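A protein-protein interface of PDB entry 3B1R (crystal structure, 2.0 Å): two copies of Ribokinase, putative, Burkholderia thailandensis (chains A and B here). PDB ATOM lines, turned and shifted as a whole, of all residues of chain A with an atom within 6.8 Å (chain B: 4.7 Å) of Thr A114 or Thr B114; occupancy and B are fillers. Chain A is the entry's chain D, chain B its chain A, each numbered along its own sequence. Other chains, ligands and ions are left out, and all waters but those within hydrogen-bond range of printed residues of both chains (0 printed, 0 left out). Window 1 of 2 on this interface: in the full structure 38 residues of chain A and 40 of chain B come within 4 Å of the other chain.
Of the 17 printed residues of chain A, 6 touch a printed residue of chain B. Along chain A the printed residues that touch a printed residue of chain B span positions 23 to 124. Of the 9 printed residues of chain B, 5 touch a printed residue of chain A. Printed residues of chain B that touch a printed residue of chain A: Met B23, Phe B29, Met B112, Thr B114 and Ile B122.
The backbone NH (N) of Met B23 sits at hydrogen-bond distance from the backbone carbonyl oxygen (O) of Ile B113 (2.7 Å). O of Met B23 lies within hydrogen-bond range of N of Thr B115 (2.9 Å). N of Met A23 lies within hydrogen-bond range of O of Ile A113. O of Met A23 lies within hydrogen-bond range of N of Thr A115, at 2.9 Å. The backbone carbonyl oxygen (O) of Ala A124 is in hydrogen-bond range of the backbone NH (N) of Met A112, at 2.9 Å. OG1 of Thr A114 is in hydrogen-bond range of O of Ile A122, at 2.7 Å.
Met A23 touches Met B112, and with the chains exchanged Met A112 touches Met B23. Thr A114 touches its own counterpart, Thr B114. Ile A122 touches Phe B29, but with the chains exchanged Phe A29 does not touch Ile B122 (4.2 Å). Of the 6 pairs that touch across the chains among the printed residues, 3 have their exchanged pair printed and touching as well.
Thr B114 touches one residue of chain A. Of the printed residues of chain B, Phe A45 touches Ile B122. Of the printed residues of chain B, Ala A124 touches Met B23 (3.8 Å). Asn B120 touches none of the printed residues of chain A. The nearest printed residue of chain B that does not touch Thr A114 is Ile B122 (4.9 Å).
Met A23 touches Met B112 (CE to CB, 3.2 Å). Phe A45 touches Ile B122 (CE1 to CG2, 3.8 Å). CE of Met B23 touches CB of Met A112, 3.9 Å away. Phe B29 touches Ile A122 (CE1 to CG2, 3.8 Å). CB of Ala A124 touches CG of Met B23 (3.8 Å).
The side-chain hydroxyl (OG1) of Thr B114 lies within hydrogen-bond range of the side-chain hydroxyl (OG1) of Thr A114 (3.2 Å).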
ATOM      1  N   ASN A  21      31.169  23.653   6.121  1.00  0.00           N
ATOM      2  CA  ASN A  21      29.738  23.458   6.323  1.00  0.00           C
ATOM      3  C   ASN A  21      29.277  22.419   5.337  1.00  0.00           C
ATOM      4  O   ASN A  21      29.133  22.689   4.145  1.00  0.00           O
ATOM      5  CB  ASN A  21      28.986  24.764   6.142  1.00  0.00           C
ATOM      6  CG  ASN A  21      29.670  25.897   6.837  1.00  0.00           C
ATOM      7  OD1 ASN A  21      30.744  26.333   6.418  1.00  0.00           O
ATOM      8  ND2 ASN A  21      29.081  26.367   7.930  1.00  0.00           N
ATOM      9  N   ILE A  22      29.087  21.206   5.836  1.00  0.00           N
ATOM     10  CA  ILE A  22      28.831  20.084   4.966  1.00  0.00           C
ATOM     11  C   ILE A  22      27.380  19.639   5.031  1.00  0.00           C
ATOM     12  O   ILE A  22      26.821  19.400   6.110  1.00  0.00           O
ATOM     13  CB  ILE A  22      29.762  18.890   5.255  1.00  0.00           C
ATOM     14  CG1 ILE A  22      31.235  19.296   5.073  1.00  0.00           C
ATOM     15  CG2 ILE A  22      29.426  17.733   4.309  1.00  0.00           C
ATOM     16  CD1 ILE A  22      32.236  18.489   5.940  1.00  0.00           C
ATOM     17  N   MET A  23      26.802  19.528   3.849  1.00  0.00           N
ATOM     18  CA  MET A  23      25.440  19.082   3.666  1.00  0.00           C
ATOM     19  C   MET A  23      25.498  17.777   2.874  1.00  0.00           C
ATOM     20  O   MET A  23      25.523  17.779   1.643  1.00  0.00           O
ATOM     21  CB  MET A  23      24.658  20.179   2.942  1.00  0.00           C
ATOM     22  CG  MET A  23      24.717  21.539   3.697  1.00  0.00           C
ATOM     23  SD  MET A  23      24.941  23.036   2.708  1.00  0.00           S
ATOM     24  CE  MET A  23      23.543  22.945   1.618  1.00  0.00           C
ATOM     25  N   THR A  24      25.557  16.659   3.595  1.00  0.00           N
ATOM     26  CA  THR A  24      25.668  15.349   2.956  1.00  0.00           C
ATOM     27  C   THR A  24      24.305  14.748   2.715  1.00  0.00           C
ATOM     28  O   THR A  24      23.562  14.460   3.661  1.00  0.00           O
ATOM     29  CB  THR A  24      26.467  14.325   3.796  1.00  0.00           C
ATOM     30  OG1 THR A  24      27.740  14.871   4.168  1.00  0.00           O
ATOM     31  CG2 THR A  24      26.676  13.023   2.990  1.00  0.00           C
ATOM     32  N   PHE A  25      23.992  14.544   1.444  1.00  0.00           N
ATOM     33  CA  PHE A  25      22.800  13.816   1.073  1.00  0.00           C
ATOM     34  C   PHE A  25      22.976  12.389   1.581  1.00  0.00           C
ATOM     35  O   PHE A  25      23.996  11.737   1.300  1.00  0.00           O
ATOM     36  CB  PHE A  25      22.604  13.850  -0.437  1.00  0.00           C
ATOM     37  CG  PHE A  25      21.377  13.123  -0.915  1.00  0.00           C
ATOM     38  CD1 PHE A  25      20.124  13.394  -0.368  1.00  0.00           C
ATOM     39  CD2 PHE A  25      21.473  12.193  -1.934  1.00  0.00           C
ATOM     40  CE1 PHE A  25      18.988  12.726  -0.820  1.00  0.00           C
ATOM     41  CE2 PHE A  25      20.344  11.525  -2.388  1.00  0.00           C
ATOM     42  CZ  PHE A  25      19.104  11.792  -1.832  1.00  0.00           C
ATOM     43  N   PHE A  29      23.707  10.877  -5.511  1.00  0.00           N
ATOM     44  CA  PHE A  29      23.199  11.700  -6.613  1.00  0.00           C
ATOM     45  C   PHE A  29      23.001  10.891  -7.887  1.00  0.00           C
ATOM     46  O   PHE A  29      22.088  11.163  -8.663  1.00  0.00           O
ATOM     47  CB  PHE A  29      24.138  12.884  -6.901  1.00  0.00           C
ATOM     48  CG  PHE A  29      24.297  13.842  -5.749  1.00  0.00           C
ATOM     49  CD1 PHE A  29      23.292  13.997  -4.797  1.00  0.00           C
ATOM     50  CD2 PHE A  29      25.443  14.621  -5.642  1.00  0.00           C
ATOM     51  CE1 PHE A  29      23.437  14.903  -3.728  1.00  0.00           C
ATOM     52  CE2 PHE A  29      25.603  15.528  -4.593  1.00  0.00           C
ATOM     53  CZ  PHE A  29      24.598  15.671  -3.630  1.00  0.00           C
ATOM     54  N   PHE A  45      16.476  17.940   0.549  1.00  0.00           N
ATOM     55  CA  PHE A  45      16.553  16.946   1.608  1.00  0.00           C
ATOM     56  C   PHE A  45      16.675  17.582   2.981  1.00  0.00           C
ATOM     57  O   PHE A  45      17.366  18.596   3.152  1.00  0.00           O
ATOM     58  CB  PHE A  45      17.700  15.957   1.359  1.00  0.00           C
ATOM     59  CG  PHE A  45      19.046  16.606   1.148  1.00  0.00           C
ATOM     60  CD1 PHE A  45      19.428  17.059  -0.109  1.00  0.00           C
ATOM     61  CD2 PHE A  45      19.941  16.737   2.201  1.00  0.00           C
ATOM     62  CE1 PHE A  45      20.675  17.666  -0.310  1.00  0.00           C
ATOM     63  CE2 PHE A  45      21.193  17.332   2.007  1.00  0.00           C
ATOM     64  CZ  PHE A  45      21.556  17.795   0.745  1.00  0.00           C
ATOM     65  N   MET A 112      31.019  25.784   1.713  1.00  0.00           N
ATOM     66  CA  MET A 112      29.691  25.171   1.747  1.00  0.00           C
ATOM     67  C   MET A 112      29.708  23.968   0.826  1.00  0.00           C
ATOM     68  O   MET A 112      29.699  24.111  -0.388  1.00  0.00           O
ATOM     69  CB  MET A 112      28.597  26.157   1.327  1.00  0.00           C
ATOM     70  CG  MET A 112      28.214  27.153   2.392  1.00  0.00           C
ATOM     71  SD  MET A 112      29.434  28.466   2.600  1.00  0.00           S
ATOM     72  CE  MET A 112      30.035  28.171   4.256  1.00  0.00           C
ATOM     73  N   ILE A 113      29.745  22.779   1.415  1.00  0.00           N
ATOM     74  CA  ILE A 113      29.931  21.560   0.643  1.00  0.00           C
ATOM     75  C   ILE A 113      28.654  20.740   0.604  1.00  0.00           C
ATOM     76  O   ILE A 113      28.169  20.261   1.628  1.00  0.00           O
ATOM     77  CB  ILE A 113      31.070  20.688   1.193  1.00  0.00           C
ATOM     78  CG1 ILE A 113      32.376  21.484   1.303  1.00  0.00           C
ATOM     79  CG2 ILE A 113      31.274  19.468   0.286  1.00  0.00           C
ATOM     80  CD1 ILE A 113      33.470  20.744   2.026  1.00  0.00           C
ATOM     81  N   THR A 114      28.123  20.568  -0.598  1.00  0.00           N
ATOM     82  CA  THR A 114      26.950  19.739  -0.783  1.00  0.00           C
ATOM     83  C   THR A 114      27.384  18.425  -1.398  1.00  0.00           C
ATOM     84  O   THR A 114      28.009  18.398  -2.458  1.00  0.00           O
ATOM     85  CB  THR A 114      25.901  20.456  -1.633  1.00  0.00           C
ATOM     86  OG1 THR A 114      26.555  21.074  -2.730  1.00  0.00           O
ATOM     87  CG2 THR A 114      25.241  21.543  -0.817  1.00  0.00           C
ATOM     88  N   THR A 115      27.086  17.330  -0.705  1.00  0.00           N
ATOM     89  CA  THR A 115      27.642  16.037  -1.095  1.00  0.00           C
ATOM     90  C   THR A 115      26.681  14.872  -0.940  1.00  0.00           C
ATOM     91  O   THR A 115      25.506  15.047  -0.607  1.00  0.00           O
ATOM     92  CB  THR A 115      28.912  15.715  -0.290  1.00  0.00           C
ATOM     93  OG1 THR A 115      29.521  16.937   0.145  1.00  0.00           O
ATOM     94  CG2 THR A 115      29.891  14.940  -1.140  1.00  0.00           C
ATOM     95  N   ASP A 116      27.213  13.684  -1.212  1.00  0.00           N
ATOM     96  CA  ASP A 116      26.495  12.438  -1.121  1.00  0.00           C
ATOM     97  C   ASP A 116      27.488  11.384  -0.662  1.00  0.00           C
ATOM     98  O   ASP A 116      28.672  11.694  -0.477  1.00  0.00           O
ATOM     99  CB  ASP A 116      25.836  12.091  -2.462  1.00  0.00           C
ATOM    100  CG  ASP A 116      26.834  11.759  -3.560  1.00  0.00           C
ATOM    101  OD1 ASP A 116      28.070  11.839  -3.341  1.00  0.00           O
ATOM    102  OD2 ASP A 116      26.364  11.419  -4.662  1.00  0.00           O
ATOM    103  N   ASN A 120      30.650  12.991  -4.122  1.00  0.00           N
ATOM    104  CA  ASN A 120      30.435  13.950  -5.185  1.00  0.00           C
ATOM    105  C   ASN A 120      30.313  15.366  -4.588  1.00  0.00           C
ATOM    106  O   ASN A 120      29.205  15.886  -4.429  1.00  0.00           O
ATOM    107  CB  ASN A 120      29.184  13.563  -5.974  1.00  0.00           C
ATOM    108  CG  ASN A 120      29.371  12.278  -6.793  1.00  0.00           C
ATOM    109  OD1 ASN A 120      30.494  11.908  -7.140  1.00  0.00           O
ATOM    110  ND2 ASN A 120      28.262  11.608  -7.116  1.00  0.00           N
ATOM    111  N   GLN A 121      31.448  15.973  -4.234  1.00  0.00           N
ATOM    112  CA  GLN A 121      31.449  17.292  -3.581  1.00  0.00           C
ATOM    113  C   GLN A 121      31.201  18.408  -4.585  1.00  0.00           C
ATOM    114  O   GLN A 121      31.977  18.592  -5.515  1.00  0.00           O
ATOM    115  CB  GLN A 121      32.763  17.557  -2.818  1.00  0.00           C
ATOM    116  CG  GLN A 121      33.139  16.486  -1.794  1.00  0.00           C
ATOM    117  CD  GLN A 121      34.482  16.713  -1.122  1.00  0.00           C
ATOM    118  OE1 GLN A 121      34.976  17.842  -1.029  1.00  0.00           O
ATOM    119  NE2 GLN A 121      35.074  15.635  -0.625  1.00  0.00           N
ATOM    120  N   ILE A 122      30.102  19.140  -4.396  1.00  0.00           N
ATOM    121  CA  ILE A 122      29.826  20.377  -5.126  1.00  0.00           C
ATOM    122  C   ILE A 122      29.930  21.508  -4.106  1.00  0.00           C
ATOM    123  O   ILE A 122      29.121  21.613  -3.179  1.00  0.00           O
ATOM    124  CB  ILE A 122      28.448  20.367  -5.802  1.00  0.00           C
ATOM    125  CG1 ILE A 122      28.296  19.117  -6.683  1.00  0.00           C
ATOM    126  CG2 ILE A 122      28.205  21.667  -6.599  1.00  0.00           C
ATOM    127  CD1 ILE A 122      26.901  18.903  -7.220  1.00  0.00           C
ATOM    128  N   THR A 123      30.945  22.346  -4.273  1.00  0.00           N
ATOM    129  CA  THR A 123      31.341  23.259  -3.213  1.00  0.00           C
ATOM    130  C   THR A 123      31.340  24.694  -3.677  1.00  0.00           C
ATOM    131  O   THR A 123      31.862  25.000  -4.740  1.00  0.00           O
ATOM    132  CB  THR A 123      32.750  22.889  -2.690  1.00  0.00           C
ATOM    133  OG1 THR A 123      32.720  21.549  -2.207  1.00  0.00           O
ATOM    134  CG2 THR A 123      33.214  23.815  -1.567  1.00  0.00           C
ATOM    135  N   ALA A 124      30.737  25.563  -2.868  1.00  0.00           N
ATOM    136  CA  ALA A 124      30.887  26.997  -3.004  1.00  0.00           C
ATOM    137  C   ALA A 124      31.901  27.454  -1.944  1.00  0.00           C
ATOM    138  O   ALA A 124      31.710  27.239  -0.744  1.00  0.00           O
ATOM    139  CB  ALA A 124      29.541  27.712  -2.841  1.00  0.00           C
ATOM    140  N   MET B  23      23.617  29.289  -3.816  1.00  0.00           N
ATOM    141  CA  MET B  23      24.931  29.179  -4.414  1.00  0.00           C
ATOM    142  C   MET B  23      24.804  28.665  -5.848  1.00  0.00           C
ATOM    143  O   MET B  23      24.663  27.460  -6.081  1.00  0.00           O
ATOM    144  CB  MET B  23      25.825  28.252  -3.578  1.00  0.00           C
ATOM    145  CG  MET B  23      25.984  28.668  -2.102  1.00  0.00           C
ATOM    146  SD  MET B  23      24.575  28.249  -1.032  1.00  0.00           S
ATOM    147  CE  MET B  23      25.120  26.736  -0.252  1.00  0.00           C
ATOM    148  N   PHE B  29      25.966  21.679 -14.497  1.00  0.00           N
ATOM    149  CA  PHE B  29      26.418  20.460 -13.824  1.00  0.00           C
ATOM    150  C   PHE B  29      26.603  19.330 -14.833  1.00  0.00           C
ATOM    151  O   PHE B  29      27.517  18.498 -14.700  1.00  0.00           O
ATOM    152  CB  PHE B  29      25.413  20.012 -12.755  1.00  0.00           C
ATOM    153  CG  PHE B  29      25.356  20.899 -11.531  1.00  0.00           C
ATOM    154  CD1 PHE B  29      26.473  21.577 -11.078  1.00  0.00           C
ATOM    155  CD2 PHE B  29      24.175  20.995 -10.791  1.00  0.00           C
ATOM    156  CE1 PHE B  29      26.415  22.369  -9.930  1.00  0.00           C
ATOM    157  CE2 PHE B  29      24.104  21.790  -9.646  1.00  0.00           C
ATOM    158  CZ  PHE B  29      25.234  22.475  -9.216  1.00  0.00           C
ATOM    159  N   MET B 112      19.136  25.889   1.953  1.00  0.00           N
ATOM    160  CA  MET B 112      20.498  26.009   1.458  1.00  0.00           C
ATOM    161  C   MET B 112      20.511  25.414   0.069  1.00  0.00           C
ATOM    162  O   MET B 112      20.494  24.196  -0.097  1.00  0.00           O
ATOM    163  CB  MET B 112      21.491  25.276   2.360  1.00  0.00           C
ATOM    164  CG  MET B 112      22.262  26.173   3.285  1.00  0.00           C
ATOM    165  SD  MET B 112      21.201  26.893   4.536  1.00  0.00           S
ATOM    166  CE  MET B 112      22.354  27.986   5.366  1.00  0.00           C
ATOM    167  N   ILE B 113      20.510  26.287  -0.926  1.00  0.00           N
ATOM    168  CA  ILE B 113      20.314  25.856  -2.303  1.00  0.00           C
ATOM    169  C   ILE B 113      21.612  25.977  -3.076  1.00  0.00           C
ATOM    170  O   ILE B 113      22.164  27.067  -3.210  1.00  0.00           O
ATOM    171  CB  ILE B 113      19.212  26.683  -3.025  1.00  0.00           C
ATOM    172  CG1 ILE B 113      17.883  26.619  -2.254  1.00  0.00           C
ATOM    173  CG2 ILE B 113      19.036  26.172  -4.460  1.00  0.00           C
ATOM    174  CD1 ILE B 113      16.888  27.761  -2.586  1.00  0.00           C
ATOM    175  N   THR B 114      22.089  24.854  -3.601  1.00  0.00           N
ATOM    176  CA  THR B 114      23.219  24.901  -4.523  1.00  0.00           C
ATOM    177  C   THR B 114      22.740  24.431  -5.890  1.00  0.00           C
ATOM    178  O   THR B 114      22.065  23.399  -6.015  1.00  0.00           O
ATOM    179  CB  THR B 114      24.426  24.103  -4.008  1.00  0.00           C
ATOM    180  OG1 THR B 114      24.015  22.782  -3.667  1.00  0.00           O
ATOM    181  CG2 THR B 114      24.975  24.740  -2.780  1.00  0.00           C
ATOM    182  N   THR B 115      23.042  25.219  -6.907  1.00  0.00           N
ATOM    183  CA  THR B 115      22.399  25.036  -8.192  1.00  0.00           C
ATOM    184  C   THR B 115      23.336  25.381  -9.346  1.00  0.00           C
ATOM    185  O   THR B 115      24.497  25.745  -9.128  1.00  0.00           O
ATOM    186  CB  THR B 115      21.064  25.836  -8.232  1.00  0.00           C
ATOM    187  OG1 THR B 115      20.439  25.710  -9.520  1.00  0.00           O
ATOM    188  CG2 THR B 115      21.284  27.308  -7.903  1.00  0.00           C
ATOM    189  N   ASN B 120      19.236  22.926 -11.814  1.00  0.00           N
ATOM    190  CA  ASN B 120      19.404  21.707 -11.044  1.00  0.00           C
ATOM    191  C   ASN B 120      19.624  22.031  -9.553  1.00  0.00           C
ATOM    192  O   ASN B 120      20.754  21.954  -9.033  1.00  0.00           O
ATOM    193  CB  ASN B 120      20.549  20.851 -11.619  1.00  0.00           C
ATOM    194  CG  ASN B 120      20.202  20.240 -12.972  1.00  0.00           C
ATOM    195  OD1 ASN B 120      19.159  19.611 -13.135  1.00  0.00           O
ATOM    196  ND2 ASN B 120      21.088  20.410 -13.946  1.00  0.00           N
ATOM    197  N   GLN B 121      18.538  22.385  -8.867  1.00  0.00           N
ATOM    198  CA  GLN B 121      18.595  22.736  -7.450  1.00  0.00           C
ATOM    199  C   GLN B 121      18.754  21.514  -6.577  1.00  0.00           C
ATOM    200  O   GLN B 121      17.901  20.613  -6.587  1.00  0.00           O
ATOM    201  CB  GLN B 121      17.328  23.462  -7.023  1.00  0.00           C
ATOM    202  CG  GLN B 121      17.094  24.760  -7.729  1.00  0.00           C
ATOM    203  CD  GLN B 121      15.862  25.458  -7.234  1.00  0.00           C
ATOM    204  OE1 GLN B 121      15.576  25.462  -6.038  1.00  0.00           O
ATOM    205  NE2 GLN B 121      15.128  26.084  -8.153  1.00  0.00           N
ATOM    206  N   ILE B 122      19.853  21.494  -5.832  1.00  0.00           N
ATOM    207  CA  ILE B 122      20.094  20.494  -4.798  1.00  0.00           C
ATOM    208  C   ILE B 122      20.016  21.229  -3.481  1.00  0.00           C
ATOM    209  O   ILE B 122      20.900  22.007  -3.143  1.00  0.00           O
ATOM    210  CB  ILE B 122      21.471  19.799  -4.965  1.00  0.00           C
ATOM    211  CG1 ILE B 122      21.589  19.204  -6.376  1.00  0.00           C
ATOM    212  CG2 ILE B 122      21.697  18.759  -3.842  1.00  0.00           C
ATOM    213  CD1 ILE B 122      22.881  18.424  -6.650  1.00  0.00           C
